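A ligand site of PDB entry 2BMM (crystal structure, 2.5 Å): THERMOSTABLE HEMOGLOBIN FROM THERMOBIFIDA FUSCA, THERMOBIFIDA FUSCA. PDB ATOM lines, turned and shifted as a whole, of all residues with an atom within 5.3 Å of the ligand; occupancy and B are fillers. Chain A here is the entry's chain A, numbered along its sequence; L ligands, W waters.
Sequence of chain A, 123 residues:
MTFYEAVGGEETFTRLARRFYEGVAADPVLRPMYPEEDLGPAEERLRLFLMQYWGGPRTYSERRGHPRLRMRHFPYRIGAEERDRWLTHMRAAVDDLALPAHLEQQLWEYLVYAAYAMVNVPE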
ATOM      1  N   TYR A  21       7.820 -25.189   0.856  1.00  0.00           N
ATOM      2  CA  TYR A  21       8.486 -26.343   0.254  1.00  0.00           C
ATOM      3  C   TYR A  21       8.603 -26.346  -1.264  1.00  0.00           C
ATOM      4  O   TYR A  21       9.585 -26.854  -1.805  1.00  0.00           O
ATOM      5  CB  TYR A  21       7.917 -27.651   0.798  1.00  0.00           C
ATOM      6  CG  TYR A  21       8.828 -28.214   1.853  1.00  0.00           C
ATOM      7  CD1 TYR A  21       8.609 -27.942   3.208  1.00  0.00           C
ATOM      8  CD2 TYR A  21       9.938 -28.982   1.499  1.00  0.00           C
ATOM      9  CE1 TYR A  21       9.462 -28.440   4.184  1.00  0.00           C
ATOM     10  CE2 TYR A  21      10.782 -29.472   2.454  1.00  0.00           C
ATOM     11  CZ  TYR A  21      10.545 -29.206   3.796  1.00  0.00           C
ATOM     12  OH  TYR A  21      11.410 -29.732   4.744  1.00  0.00           O
ATOM     13  N   LEU A  30      19.509 -25.054  -1.299  1.00  0.00           N
ATOM     14  CA  LEU A  30      18.764 -25.752  -0.260  1.00  0.00           C
ATOM     15  C   LEU A  30      18.323 -27.166  -0.609  1.00  0.00           C
ATOM     16  O   LEU A  30      18.459 -28.068   0.221  1.00  0.00           O
ATOM     17  CB  LEU A  30      17.571 -24.931   0.203  1.00  0.00           C
ATOM     18  CG  LEU A  30      17.923 -23.623   0.932  1.00  0.00           C
ATOM     19  CD1 LEU A  30      16.626 -23.046   1.418  1.00  0.00           C
ATOM     20  CD2 LEU A  30      18.920 -23.827   2.093  1.00  0.00           C
ATOM     21  N   MET A  33      20.250 -30.303   0.114  1.00  0.00           N
ATOM     22  CA  MET A  33      20.407 -30.384   1.560  1.00  0.00           C
ATOM     23  C   MET A  33      19.278 -31.135   2.240  1.00  0.00           C
ATOM     24  O   MET A  33      19.449 -31.678   3.310  1.00  0.00           O
ATOM     25  CB  MET A  33      20.505 -28.993   2.152  1.00  0.00           C
ATOM     26  CG  MET A  33      21.651 -28.224   1.606  1.00  0.00           C
ATOM     27  SD  MET A  33      22.194 -26.955   2.755  1.00  0.00           S
ATOM     28  CE  MET A  33      22.127 -27.849   4.324  1.00  0.00           C
ATOM     29  N   TYR A  34      18.108 -31.158   1.618  1.00  0.00           N
ATOM     30  CA  TYR A  34      17.051 -32.020   2.085  1.00  0.00           C
ATOM     31  C   TYR A  34      17.317 -33.366   1.424  1.00  0.00           C
ATOM     32  O   TYR A  34      17.106 -33.521   0.221  1.00  0.00           O
ATOM     33  CB  TYR A  34      15.675 -31.437   1.742  1.00  0.00           C
ATOM     34  CG  TYR A  34      15.432 -30.124   2.447  1.00  0.00           C
ATOM     35  CD1 TYR A  34      16.176 -29.001   2.129  1.00  0.00           C
ATOM     36  CD2 TYR A  34      14.462 -30.015   3.440  1.00  0.00           C
ATOM     37  CE1 TYR A  34      15.998 -27.807   2.760  1.00  0.00           C
ATOM     38  CE2 TYR A  34      14.267 -28.815   4.100  1.00  0.00           C
ATOM     39  CZ  TYR A  34      15.034 -27.717   3.745  1.00  0.00           C
ATOM     40  OH  TYR A  34      14.863 -26.502   4.358  1.00  0.00           O
ATOM     41  N   PRO A  35      17.833 -34.333   2.217  1.00  0.00           N
ATOM     42  CA  PRO A  35      18.436 -35.535   1.636  1.00  0.00           C
ATOM     43  C   PRO A  35      17.392 -36.595   1.235  1.00  0.00           C
ATOM     44  O   PRO A  35      17.736 -37.763   1.000  1.00  0.00           O
ATOM     45  CB  PRO A  35      19.358 -36.061   2.763  1.00  0.00           C
ATOM     46  CG  PRO A  35      19.063 -35.203   3.971  1.00  0.00           C
ATOM     47  CD  PRO A  35      17.851 -34.378   3.694  1.00  0.00           C
ATOM     48  N   GLU A  36      16.129 -36.181   1.148  1.00  0.00           N
ATOM     49  CA  GLU A  36      15.116 -37.110   0.722  1.00  0.00           C
ATOM     50  C   GLU A  36      14.866 -36.963  -0.787  1.00  0.00           C
ATOM     51  O   GLU A  36      14.825 -35.850  -1.308  1.00  0.00           O
ATOM     52  CB  GLU A  36      13.844 -36.930   1.572  1.00  0.00           C
ATOM     53  CG  GLU A  36      14.035 -37.280   3.072  1.00  0.00           C
ATOM     54  CD  GLU A  36      12.742 -37.137   3.918  1.00  0.00           C
ATOM     55  OE1 GLU A  36      11.777 -36.437   3.474  1.00  0.00           O
ATOM     56  OE2 GLU A  36      12.675 -37.713   5.035  1.00  0.00           O
ATOM     57  N   LEU A  39      10.110 -35.221  -0.815  1.00  0.00           N
ATOM     58  CA  LEU A  39      10.003 -34.152   0.210  1.00  0.00           C
ATOM     59  C   LEU A  39       8.648 -34.061   0.936  1.00  0.00           C
ATOM     60  O   LEU A  39       8.394 -33.112   1.686  1.00  0.00           O
ATOM     61  CB  LEU A  39      10.317 -32.790  -0.410  1.00  0.00           C
ATOM     62  CG  LEU A  39      11.792 -32.503  -0.651  1.00  0.00           C
ATOM     63  CD1 LEU A  39      11.937 -31.045  -1.011  1.00  0.00           C
ATOM     64  CD2 LEU A  39      12.648 -32.879   0.579  1.00  0.00           C
ATOM     65  N   ALA A  42       8.800 -34.503   4.894  1.00  0.00           N
ATOM     66  CA  ALA A  42       9.490 -33.357   5.477  1.00  0.00           C
ATOM     67  C   ALA A  42       8.480 -32.217   5.596  1.00  0.00           C
ATOM     68  O   ALA A  42       8.309 -31.671   6.677  1.00  0.00           O
ATOM     69  CB  ALA A  42      10.705 -32.961   4.655  1.00  0.00           C
ATOM     70  N   ARG A  45       6.176 -32.891   8.381  1.00  0.00           N
ATOM     71  CA  ARG A  45       6.766 -32.651   9.701  1.00  0.00           C
ATOM     72  C   ARG A  45       6.725 -31.159  10.052  1.00  0.00           C
ATOM     73  O   ARG A  45       6.357 -30.800  11.184  1.00  0.00           O
ATOM     74  CB  ARG A  45       8.185 -33.228   9.817  1.00  0.00           C
ATOM     75  CG  ARG A  45       8.194 -34.731  10.068  1.00  0.00           C
ATOM     76  CD  ARG A  45       9.596 -35.292  10.193  1.00  0.00           C
ATOM     77  NE  ARG A  45       9.651 -36.632   9.603  1.00  0.00           N
ATOM     78  CZ  ARG A  45      10.011 -36.893   8.339  1.00  0.00           C
ATOM     79  NH1 ARG A  45      10.394 -35.912   7.533  1.00  0.00           N
ATOM     80  NH2 ARG A  45       9.989 -38.135   7.880  1.00  0.00           N
ATOM     81  N   LEU A  46       7.071 -30.297   9.078  1.00  0.00           N
ATOM     82  CA  LEU A  46       7.035 -28.861   9.278  1.00  0.00           C
ATOM     83  C   LEU A  46       5.610 -28.427   9.623  1.00  0.00           C
ATOM     84  O   LEU A  46       5.363 -27.871  10.704  1.00  0.00           O
ATOM     85  CB  LEU A  46       7.519 -28.125   8.020  1.00  0.00           C
ATOM     86  CG  LEU A  46       8.384 -26.871   8.206  1.00  0.00           C
ATOM     87  CD1 LEU A  46       8.086 -25.823   7.132  1.00  0.00           C
ATOM     88  CD2 LEU A  46       8.267 -26.260   9.589  1.00  0.00           C
ATOM     89  N   PHE A  49       4.622 -29.384  12.888  1.00  0.00           N
ATOM     90  CA  PHE A  49       5.365 -28.707  13.920  1.00  0.00           C
ATOM     91  C   PHE A  49       4.807 -27.287  14.146  1.00  0.00           C
ATOM     92  O   PHE A  49       4.589 -26.866  15.280  1.00  0.00           O
ATOM     93  CB  PHE A  49       6.864 -28.643  13.640  1.00  0.00           C
ATOM     94  CG  PHE A  49       7.548 -27.605  14.474  1.00  0.00           C
ATOM     95  CD1 PHE A  49       7.847 -27.869  15.788  1.00  0.00           C
ATOM     96  CD2 PHE A  49       7.763 -26.329  13.971  1.00  0.00           C
ATOM     97  CE1 PHE A  49       8.421 -26.881  16.606  1.00  0.00           C
ATOM     98  CE2 PHE A  49       8.318 -25.347  14.786  1.00  0.00           C
ATOM     99  CZ  PHE A  49       8.642 -25.624  16.103  1.00  0.00           C
ATOM    100  N   LEU A  50       4.570 -26.574  13.067  1.00  0.00           N
ATOM    101  CA  LEU A  50       4.123 -25.221  13.157  1.00  0.00           C
ATOM    102  C   LEU A  50       2.744 -25.159  13.809  1.00  0.00           C
ATOM    103  O   LEU A  50       2.439 -24.263  14.652  1.00  0.00           O
ATOM    104  CB  LEU A  50       4.146 -24.603  11.762  1.00  0.00           C
ATOM    105  CG  LEU A  50       5.533 -24.309  11.175  1.00  0.00           C
ATOM    106  CD1 LEU A  50       5.436 -23.943   9.710  1.00  0.00           C
ATOM    107  CD2 LEU A  50       6.273 -23.206  11.927  1.00  0.00           C
ATOM    108  N   TYR A  60       2.353 -33.281  16.034  1.00  0.00           N
ATOM    109  CA  TYR A  60       3.789 -33.344  15.855  1.00  0.00           C
ATOM    110  C   TYR A  60       4.407 -34.117  17.018  1.00  0.00           C
ATOM    111  O   TYR A  60       5.042 -35.143  16.816  1.00  0.00           O
ATOM    112  CB  TYR A  60       4.430 -31.932  15.697  1.00  0.00           C
ATOM    113  CG  TYR A  60       5.944 -31.991  15.691  1.00  0.00           C
ATOM    114  CD1 TYR A  60       6.637 -32.212  14.515  1.00  0.00           C
ATOM    115  CD2 TYR A  60       6.678 -31.902  16.887  1.00  0.00           C
ATOM    116  CE1 TYR A  60       8.037 -32.311  14.502  1.00  0.00           C
ATOM    117  CE2 TYR A  60       8.088 -32.009  16.896  1.00  0.00           C
ATOM    118  CZ  TYR A  60       8.759 -32.216  15.697  1.00  0.00           C
ATOM    119  OH  TYR A  60      10.132 -32.313  15.650  1.00  0.00           O
ATOM    120  N   ARG A  64       6.522 -37.535  16.693  1.00  0.00           N
ATOM    121  CA  ARG A  64       7.941 -37.411  17.069  1.00  0.00           C
ATOM    122  C   ARG A  64       7.851 -36.865  18.455  1.00  0.00           C
ATOM    123  O   ARG A  64       6.805 -36.319  18.785  1.00  0.00           O
ATOM    124  CB  ARG A  64       8.632 -36.370  16.187  1.00  0.00           C
ATOM    125  CG  ARG A  64       7.947 -36.075  14.870  1.00  0.00           C
ATOM    126  CD  ARG A  64       8.950 -36.014  13.761  1.00  0.00           C
ATOM    127  NE  ARG A  64       9.379 -37.369  13.436  1.00  0.00           N
ATOM    128  CZ  ARG A  64      10.537 -37.715  12.892  1.00  0.00           C
ATOM    129  NH1 ARG A  64      11.466 -36.810  12.578  1.00  0.00           N
ATOM    130  NH2 ARG A  64      10.779 -39.004  12.652  1.00  0.00           N
ATOM    131  N   LEU A  69      14.552 -28.662  18.194  1.00  0.00           N
ATOM    132  CA  LEU A  69      14.856 -28.320  16.827  1.00  0.00           C
ATOM    133  C   LEU A  69      16.354 -28.130  16.608  1.00  0.00           C
ATOM    134  O   LEU A  69      16.922 -28.719  15.684  1.00  0.00           O
ATOM    135  CB  LEU A  69      14.027 -27.117  16.375  1.00  0.00           C
ATOM    136  CG  LEU A  69      12.552 -27.430  16.091  1.00  0.00           C
ATOM    137  CD1 LEU A  69      11.881 -26.328  15.318  1.00  0.00           C
ATOM    138  CD2 LEU A  69      12.477 -28.718  15.291  1.00  0.00           C
ATOM    139  N   ARG A  72      17.873 -31.328  16.221  1.00  0.00           N
ATOM    140  CA  ARG A  72      17.458 -32.106  15.064  1.00  0.00           C
ATOM    141  C   ARG A  72      18.076 -31.573  13.773  1.00  0.00           C
ATOM    142  O   ARG A  72      18.177 -32.300  12.791  1.00  0.00           O
ATOM    143  CB  ARG A  72      15.933 -32.137  14.956  1.00  0.00           C
ATOM    144  CG  ARG A  72      15.340 -33.012  16.005  1.00  0.00           C
ATOM    145  CD  ARG A  72      13.919 -32.640  16.290  1.00  0.00           C
ATOM    146  NE  ARG A  72      12.987 -33.652  15.824  1.00  0.00           N
ATOM    147  CZ  ARG A  72      12.364 -34.543  16.596  1.00  0.00           C
ATOM    148  NH1 ARG A  72      11.527 -35.396  16.044  1.00  0.00           N
ATOM    149  NH2 ARG A  72      12.554 -34.588  17.896  1.00  0.00           N
ATOM    150  N   HIS A  73      18.456 -30.299  13.798  1.00  0.00           N
ATOM    151  CA  HIS A  73      19.171 -29.652  12.704  1.00  0.00           C
ATOM    152  C   HIS A  73      20.676 -29.801  12.857  1.00  0.00           C
ATOM    153  O   HIS A  73      21.422 -29.239  12.070  1.00  0.00           O
ATOM    154  CB  HIS A  73      18.816 -28.174  12.646  1.00  0.00           C
ATOM    155  CG  HIS A  73      17.438 -27.928  12.158  1.00  0.00           C
ATOM    156  ND1 HIS A  73      16.343 -27.929  12.992  1.00  0.00           N
ATOM    157  CD2 HIS A  73      16.956 -27.722  10.909  1.00  0.00           C
ATOM    158  CE1 HIS A  73      15.246 -27.718  12.291  1.00  0.00           C
ATOM    159  NE2 HIS A  73      15.595 -27.589  11.019  1.00  0.00           N
ATOM    160  N   TYR A  76      23.084 -30.873   9.990  1.00  0.00           N
ATOM    161  CA  TYR A  76      23.121 -30.029   8.790  1.00  0.00           C
ATOM    162  C   TYR A  76      24.016 -28.812   8.838  1.00  0.00           C
ATOM    163  O   TYR A  76      24.268 -28.236   9.910  1.00  0.00           O
ATOM    164  CB  TYR A  76      21.694 -29.639   8.367  1.00  0.00           C
ATOM    165  CG  TYR A  76      20.781 -30.839   8.337  1.00  0.00           C
ATOM    166  CD1 TYR A  76      20.928 -31.822   7.380  1.00  0.00           C
ATOM    167  CD2 TYR A  76      19.784 -30.996   9.294  1.00  0.00           C
ATOM    168  CE1 TYR A  76      20.105 -32.926   7.343  1.00  0.00           C
ATOM    169  CE2 TYR A  76      18.968 -32.098   9.279  1.00  0.00           C
ATOM    170  CZ  TYR A  76      19.134 -33.066   8.304  1.00  0.00           C
ATOM    171  OH  TYR A  76      18.309 -34.170   8.287  1.00  0.00           O
ATOM    172  N   ILE A  78      24.191 -25.378   8.440  1.00  0.00           N
ATOM    173  CA  ILE A  78      23.306 -24.219   8.384  1.00  0.00           C
ATOM    174  C   ILE A  78      24.149 -22.998   8.707  1.00  0.00           C
ATOM    175  O   ILE A  78      24.475 -22.741   9.868  1.00  0.00           O
ATOM    176  CB  ILE A  78      22.101 -24.381   9.342  1.00  0.00           C
ATOM    177  CG1 ILE A  78      21.634 -25.854   9.352  1.00  0.00           C
ATOM    178  CG2 ILE A  78      20.985 -23.430   8.958  1.00  0.00           C
ATOM    179  CD1 ILE A  78      20.210 -26.080   9.773  1.00  0.00           C
ATOM    180  N   GLU A  82      22.680 -20.562   3.923  1.00  0.00           N
ATOM    181  CA  GLU A  82      21.590 -21.517   4.001  1.00  0.00           C
ATOM    182  C   GLU A  82      20.384 -20.930   4.712  1.00  0.00           C
ATOM    183  O   GLU A  82      19.244 -21.187   4.325  1.00  0.00           O
ATOM    184  CB  GLU A  82      22.041 -22.773   4.711  1.00  0.00           C
ATOM    185  CG  GLU A  82      22.983 -23.673   3.888  1.00  0.00           C
ATOM    186  CD  GLU A  82      24.428 -23.130   3.796  1.00  0.00           C
ATOM    187  OE1 GLU A  82      25.242 -23.742   3.028  1.00  0.00           O
ATOM    188  OE2 GLU A  82      24.756 -22.121   4.468  1.00  0.00           O
ATOM    189  N   ARG A  83      20.647 -20.104   5.737  1.00  0.00           N
ATOM    190  CA  ARG A  83      19.597 -19.473   6.512  1.00  0.00           C
ATOM    191  C   ARG A  83      18.859 -18.433   5.668  1.00  0.00           C
ATOM    192  O   ARG A  83      17.627 -18.371   5.674  1.00  0.00           O
ATOM    193  CB  ARG A  83      20.209 -18.825   7.777  1.00  0.00           C
ATOM    194  CG  ARG A  83      19.329 -17.807   8.529  1.00  0.00           C
ATOM    195  CD  ARG A  83      19.856 -16.383   8.415  1.00  0.00           C
ATOM    196  NE  ARG A  83      21.121 -16.208   9.103  1.00  0.00           N
ATOM    197  CZ  ARG A  83      22.062 -15.311   8.791  1.00  0.00           C
ATOM    198  NH1 ARG A  83      21.916 -14.437   7.788  1.00  0.00           N
ATOM    199  NH2 ARG A  83      23.181 -15.299   9.497  1.00  0.00           N
ATOM    200  N   TRP A  86      16.673 -20.099   3.249  1.00  0.00           N
ATOM    201  CA  TRP A  86      15.529 -20.624   3.970  1.00  0.00           C
ATOM    202  C   TRP A  86      14.529 -19.499   4.191  1.00  0.00           C
ATOM    203  O   TRP A  86      13.347 -19.660   3.909  1.00  0.00           O
ATOM    204  CB  TRP A  86      15.970 -21.222   5.301  1.00  0.00           C
ATOM    205  CG  TRP A  86      14.907 -22.025   6.061  1.00  0.00           C
ATOM    206  CD1 TRP A  86      14.756 -23.372   6.037  1.00  0.00           C
ATOM    207  CD2 TRP A  86      13.886 -21.528   6.960  1.00  0.00           C
ATOM    208  NE1 TRP A  86      13.729 -23.760   6.846  1.00  0.00           N
ATOM    209  CE2 TRP A  86      13.164 -22.652   7.422  1.00  0.00           C
ATOM    210  CE3 TRP A  86      13.521 -20.245   7.414  1.00  0.00           C
ATOM    211  CZ2 TRP A  86      12.070 -22.547   8.337  1.00  0.00           C
ATOM    212  CZ3 TRP A  86      12.434 -20.128   8.330  1.00  0.00           C
ATOM    213  CH2 TRP A  86      11.730 -21.278   8.785  1.00  0.00           C
ATOM    214  N   TYR A 110       8.849 -14.820  14.482  1.00  0.00           N
ATOM    215  CA  TYR A 110       9.210 -16.138  14.987  1.00  0.00           C
ATOM    216  C   TYR A 110      10.089 -16.914  14.004  1.00  0.00           C
ATOM    217  O   TYR A 110      11.163 -17.422  14.345  1.00  0.00           O
ATOM    218  CB  TYR A 110       7.971 -16.971  15.287  1.00  0.00           C
ATOM    219  CG  TYR A 110       8.339 -18.410  15.468  1.00  0.00           C
ATOM    220  CD1 TYR A 110       8.051 -19.356  14.479  1.00  0.00           C
ATOM    221  CD2 TYR A 110       9.053 -18.836  16.617  1.00  0.00           C
ATOM    222  CE1 TYR A 110       8.412 -20.684  14.640  1.00  0.00           C
ATOM    223  CE2 TYR A 110       9.426 -20.171  16.779  1.00  0.00           C
ATOM    224  CZ  TYR A 110       9.098 -21.076  15.775  1.00  0.00           C
ATOM    225  OH  TYR A 110       9.447 -22.387  15.914  1.00  0.00           O
ATOM    226  N   LEU A 111       9.621 -16.994  12.765  1.00  0.00           N
ATOM    227  CA  LEU A 111      10.330 -17.693  11.728  1.00  0.00           C
ATOM    228  C   LEU A 111      11.730 -17.124  11.540  1.00  0.00           C
ATOM    229  O   LEU A 111      12.737 -17.891  11.465  1.00  0.00           O
ATOM    230  CB  LEU A 111       9.489 -17.575  10.447  1.00  0.00           C
ATOM    231  CG  LEU A 111       8.510 -18.650   9.995  1.00  0.00           C
ATOM    232  CD1 LEU A 111       8.271 -19.869  10.909  1.00  0.00           C
ATOM    233  CD2 LEU A 111       7.240 -17.990   9.566  1.00  0.00           C
ATOM    234  N   ALA A 114      13.820 -18.031  14.720  1.00  0.00           N
ATOM    235  CA  ALA A 114      14.073 -19.465  14.743  1.00  0.00           C
ATOM    236  C   ALA A 114      15.192 -19.804  13.738  1.00  0.00           C
ATOM    237  O   ALA A 114      16.088 -20.600  14.041  1.00  0.00           O
ATOM    238  CB  ALA A 114      12.772 -20.238  14.490  1.00  0.00           C
ATOM    239  N   ALA A 115      15.193 -19.186  12.562  1.00  0.00           N
ATOM    240  CA  ALA A 115      16.207 -19.523  11.553  1.00  0.00           C
ATOM    241  C   ALA A 115      17.543 -18.985  11.940  1.00  0.00           C
ATOM    242  O   ALA A 115      18.553 -19.709  11.897  1.00  0.00           O
ATOM    243  CB  ALA A 115      15.818 -19.015  10.178  1.00  0.00           C
ATOM    244  N   TYR A 116      17.542 -17.719  12.366  1.00  0.00           N
ATOM    245  CA  TYR A 116      18.747 -17.098  12.918  1.00  0.00           C
ATOM    246  C   TYR A 116      19.361 -17.958  13.988  1.00  0.00           C
ATOM    247  O   TYR A 116      20.571 -18.139  13.998  1.00  0.00           O
ATOM    248  CB  TYR A 116      18.457 -15.680  13.394  1.00  0.00           C
ATOM    249  CG  TYR A 116      18.691 -14.686  12.285  1.00  0.00           C
ATOM    250  CD1 TYR A 116      19.911 -14.029  12.162  1.00  0.00           C
ATOM    251  CD2 TYR A 116      17.722 -14.458  11.320  1.00  0.00           C
ATOM    252  CE1 TYR A 116      20.161 -13.133  11.135  1.00  0.00           C
ATOM    253  CE2 TYR A 116      17.949 -13.537  10.259  1.00  0.00           C
ATOM    254  CZ  TYR A 116      19.175 -12.888  10.178  1.00  0.00           C
ATOM    255  OH  TYR A 116      19.438 -11.998   9.142  1.00  0.00           O
ATOM    256  N   MET A 118      18.770 -21.227  14.278  1.00  0.00           N
ATOM    257  CA  MET A 118      19.113 -22.539  13.739  1.00  0.00           C
ATOM    258  C   MET A 118      20.542 -22.586  13.145  1.00  0.00           C
ATOM    259  O   MET A 118      21.145 -23.647  13.091  1.00  0.00           O
ATOM    260  CB  MET A 118      18.074 -22.974  12.708  1.00  0.00           C
ATOM    261  CG  MET A 118      17.804 -24.445  12.727  1.00  0.00           C
ATOM    262  SD  MET A 118      16.814 -24.950  14.147  1.00  0.00           S
ATOM    263  CE  MET A 118      15.344 -23.965  13.905  1.00  0.00           C
ATOM    264  N   VAL A 119      21.072 -21.429  12.726  1.00  0.00           N
ATOM    265  CA  VAL A 119      22.429 -21.400  12.193  1.00  0.00           C
ATOM    266  C   VAL A 119      23.350 -22.086  13.198  1.00  0.00           C
ATOM    267  O   VAL A 119      23.315 -21.749  14.388  1.00  0.00           O
ATOM    268  CB  VAL A 119      22.919 -19.962  11.872  1.00  0.00           C
ATOM    269  CG1 VAL A 119      24.391 -19.960  11.467  1.00  0.00           C
ATOM    270  CG2 VAL A 119      22.055 -19.326  10.785  1.00  0.00           C
HETATM  271  C1  LIG L   1      14.041 -30.463   9.266  1.00  0.00           C
HETATM  272  C2  LIG L   1      17.171 -27.467   7.083  1.00  0.00           C
HETATM  273  C3  LIG L   1      15.400 -23.803   9.762  1.00  0.00           C
HETATM  274  C4  LIG L   1      11.794 -26.575  11.272  1.00  0.00           C
HETATM  275  C5  LIG L   1      15.046 -29.979   8.424  1.00  0.00           C
HETATM  276  C6  LIG L   1      15.773 -30.734   7.440  1.00  0.00           C
HETATM  277  C7  LIG L   1      16.644 -29.917   6.824  1.00  0.00           C
HETATM  278  C8  LIG L   1      16.483 -28.606   7.409  1.00  0.00           C
HETATM  279  C9  LIG L   1      17.675 -30.262   5.716  1.00  0.00           C
HETATM  280  C10 LIG L   1      15.548 -32.232   7.202  1.00  0.00           C
HETATM  281  C11 LIG L   1      14.551 -32.338   6.049  1.00  0.00           C
HETATM  282  C12 LIG L   1      14.362 -33.788   5.695  1.00  0.00           C
HETATM  283  O1  LIG L   1      14.683 -34.150   4.526  1.00  0.00           O
HETATM  284  O2  LIG L   1      13.899 -34.591   6.572  1.00  0.00           O
HETATM  285  C13 LIG L   1      16.939 -26.218   7.617  1.00  0.00           C
HETATM  286  C14 LIG L   1      17.645 -25.003   7.244  1.00  0.00           C
HETATM  287  C15 LIG L   1      17.155 -23.994   7.991  1.00  0.00           C
HETATM  288  C16 LIG L   1      16.128 -24.525   8.850  1.00  0.00           C
HETATM  289  C17 LIG L   1      18.753 -24.964   6.170  1.00  0.00           C
HETATM  290  C18 LIG L   1      17.588 -22.500   7.955  1.00  0.00           C
HETATM  291  C19 LIG L   1      17.628 -21.783   9.069  1.00  0.00           C
HETATM  292  C20 LIG L   1      14.247 -24.178  10.402  1.00  0.00           C
HETATM  293  C21 LIG L   1      13.341 -23.352  11.189  1.00  0.00           C
HETATM  294  C22 LIG L   1      12.330 -24.162  11.603  1.00  0.00           C
HETATM  295  C23 LIG L   1      12.589 -25.485  11.093  1.00  0.00           C
HETATM  296  C24 LIG L   1      13.568 -21.843  11.467  1.00  0.00           C
HETATM  297  C25 LIG L   1      11.089 -23.922  12.488  1.00  0.00           C
HETATM  298  C26 LIG L   1      10.552 -22.733  12.715  1.00  0.00           C
HETATM  299  C27 LIG L   1      12.091 -27.872  10.950  1.00  0.00           C
HETATM  300  C28 LIG L   1      11.374 -29.026  11.433  1.00  0.00           C
HETATM  301  C29 LIG L   1      12.078 -30.242  10.825  1.00  0.00           C
HETATM  302  C30 LIG L   1      13.159 -29.705  10.015  1.00  0.00           C
HETATM  303  C31 LIG L   1      10.160 -29.035  12.380  1.00  0.00           C
HETATM  304  C32 LIG L   1      11.685 -31.710  11.039  1.00  0.00           C
HETATM  305  C33 LIG L   1      11.697 -31.910  12.554  1.00  0.00           C
HETATM  306  C34 LIG L   1      11.598 -33.369  12.820  1.00  0.00           C
HETATM  307  O3  LIG L   1      12.518 -34.087  12.379  1.00  0.00           O
HETATM  308  O4  LIG L   1      10.613 -33.791  13.473  1.00  0.00           O
HETATM  309  N1  LIG L   1      15.503 -28.676   8.370  1.00  0.00           N
HETATM  310  N2  LIG L   1      16.022 -25.877   8.600  1.00  0.00           N
HETATM  311  N3  LIG L   1      13.750 -25.442  10.370  1.00  0.00           N
HETATM  312  N4  LIG L   1      13.118 -28.314  10.123  1.00  0.00           N
HETATM  313 FE1  LIG L   1      14.619 -27.027   9.470  1.00  0.00          FE
HETATM  314  O   HOH W   1      10.949 -30.333   7.531  1.00  0.00           O
HETATM  315  O   HOH W   2      15.550 -37.445   7.510  1.00  0.00           O
HETATM  316  O   HOH W   3      11.994 -33.067   7.869  1.00  0.00           O
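O of Met 33 touches C9 of the ligand, 3.3 Å away. Tyr 34 touches the ligand (CD2 to C11, 3.5 Å). Pro 35 touches the ligand. Glu 36 touches the ligand (CG to O1, 3.5 Å). Ala 42 touches the ligand (CB to C12, 3.9 Å). CD2 of Leu 46 touches C4 of the ligand, 3.9 Å away. Phe 49 touches the ligand. Leu 69 touches the ligand (CD2 to C31, 3.7 Å). Tyr 76 touches the ligand (OH to C10, 3.5 Å). Ile 78 touches the ligand. Arg 83 touches the ligand (CA to C18, 3.9 Å). CD1 of Trp 86 touches C15 of the ligand, 3.2 Å away. Tyr 110 touches the ligand. Ala 114 touches the ligand (C to C24, 3.5 Å). N of Ala 115 touches C24 of the ligand, 3.3 Å away. Met 118 touches the ligand. Hydrophobic or aromatic side chains that line the ligand: Tyr 34, Pro 35, Ala 42, Leu 46, Phe 49, Tyr 60, Leu 69, His 73, Tyr 76, Ile 78, Trp 86, Tyr 110, Ala 114, Ala 115 and Met 118. Of the 29 residues printed, 21 come within 4 Å of the ligand.
The guanidinium group (NH1) of Arg 72 is in salt-bridge range of an oxygen (O4) of the ligand (3.2 Å). An oxygen (O3) of the ligand lies within salt-bridge range of the guanidinium group (NH1) of Arg 64 (2.9 Å). O4 of the ligand lies within hydrogen-bond range of OH of Tyr 60 (2.7 Å). A ring nitrogen (NE2) of His 73 binds an iron atom (FE1) of the ligand, 1.9 Å away. An oxygen (O2) of the ligand is in salt-bridge range of the guanidinium group (NH1) of Arg 45 (3.9 Å).
Water W3 lies within hydrogen-bond range of O2 of the ligand and NH1 of Arg 45. Water W1 bridges OH of Tyr 21 (2.9 Å) and O of Ala 42 (3.1 Å).
NH1 of Arg 45 lies within salt-bridge range of OE2 of Glu 36 (3.8 Å). A ring nitrogen (ND1) of His 73 sits at hydrogen-bond distance from the backbone carbonyl oxygen (O) of Leu 69, 2.9 Å away. The side-chain hydroxyl (OH) of Tyr 60 sits at hydrogen-bond distance from the guanidinium group (NE) of Arg 72 (3.2 Å). A ring nitrogen (ND1) of His 73 is in hydrogen-bond range of the side-chain sulfur of Met 118 (3.2 Å).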
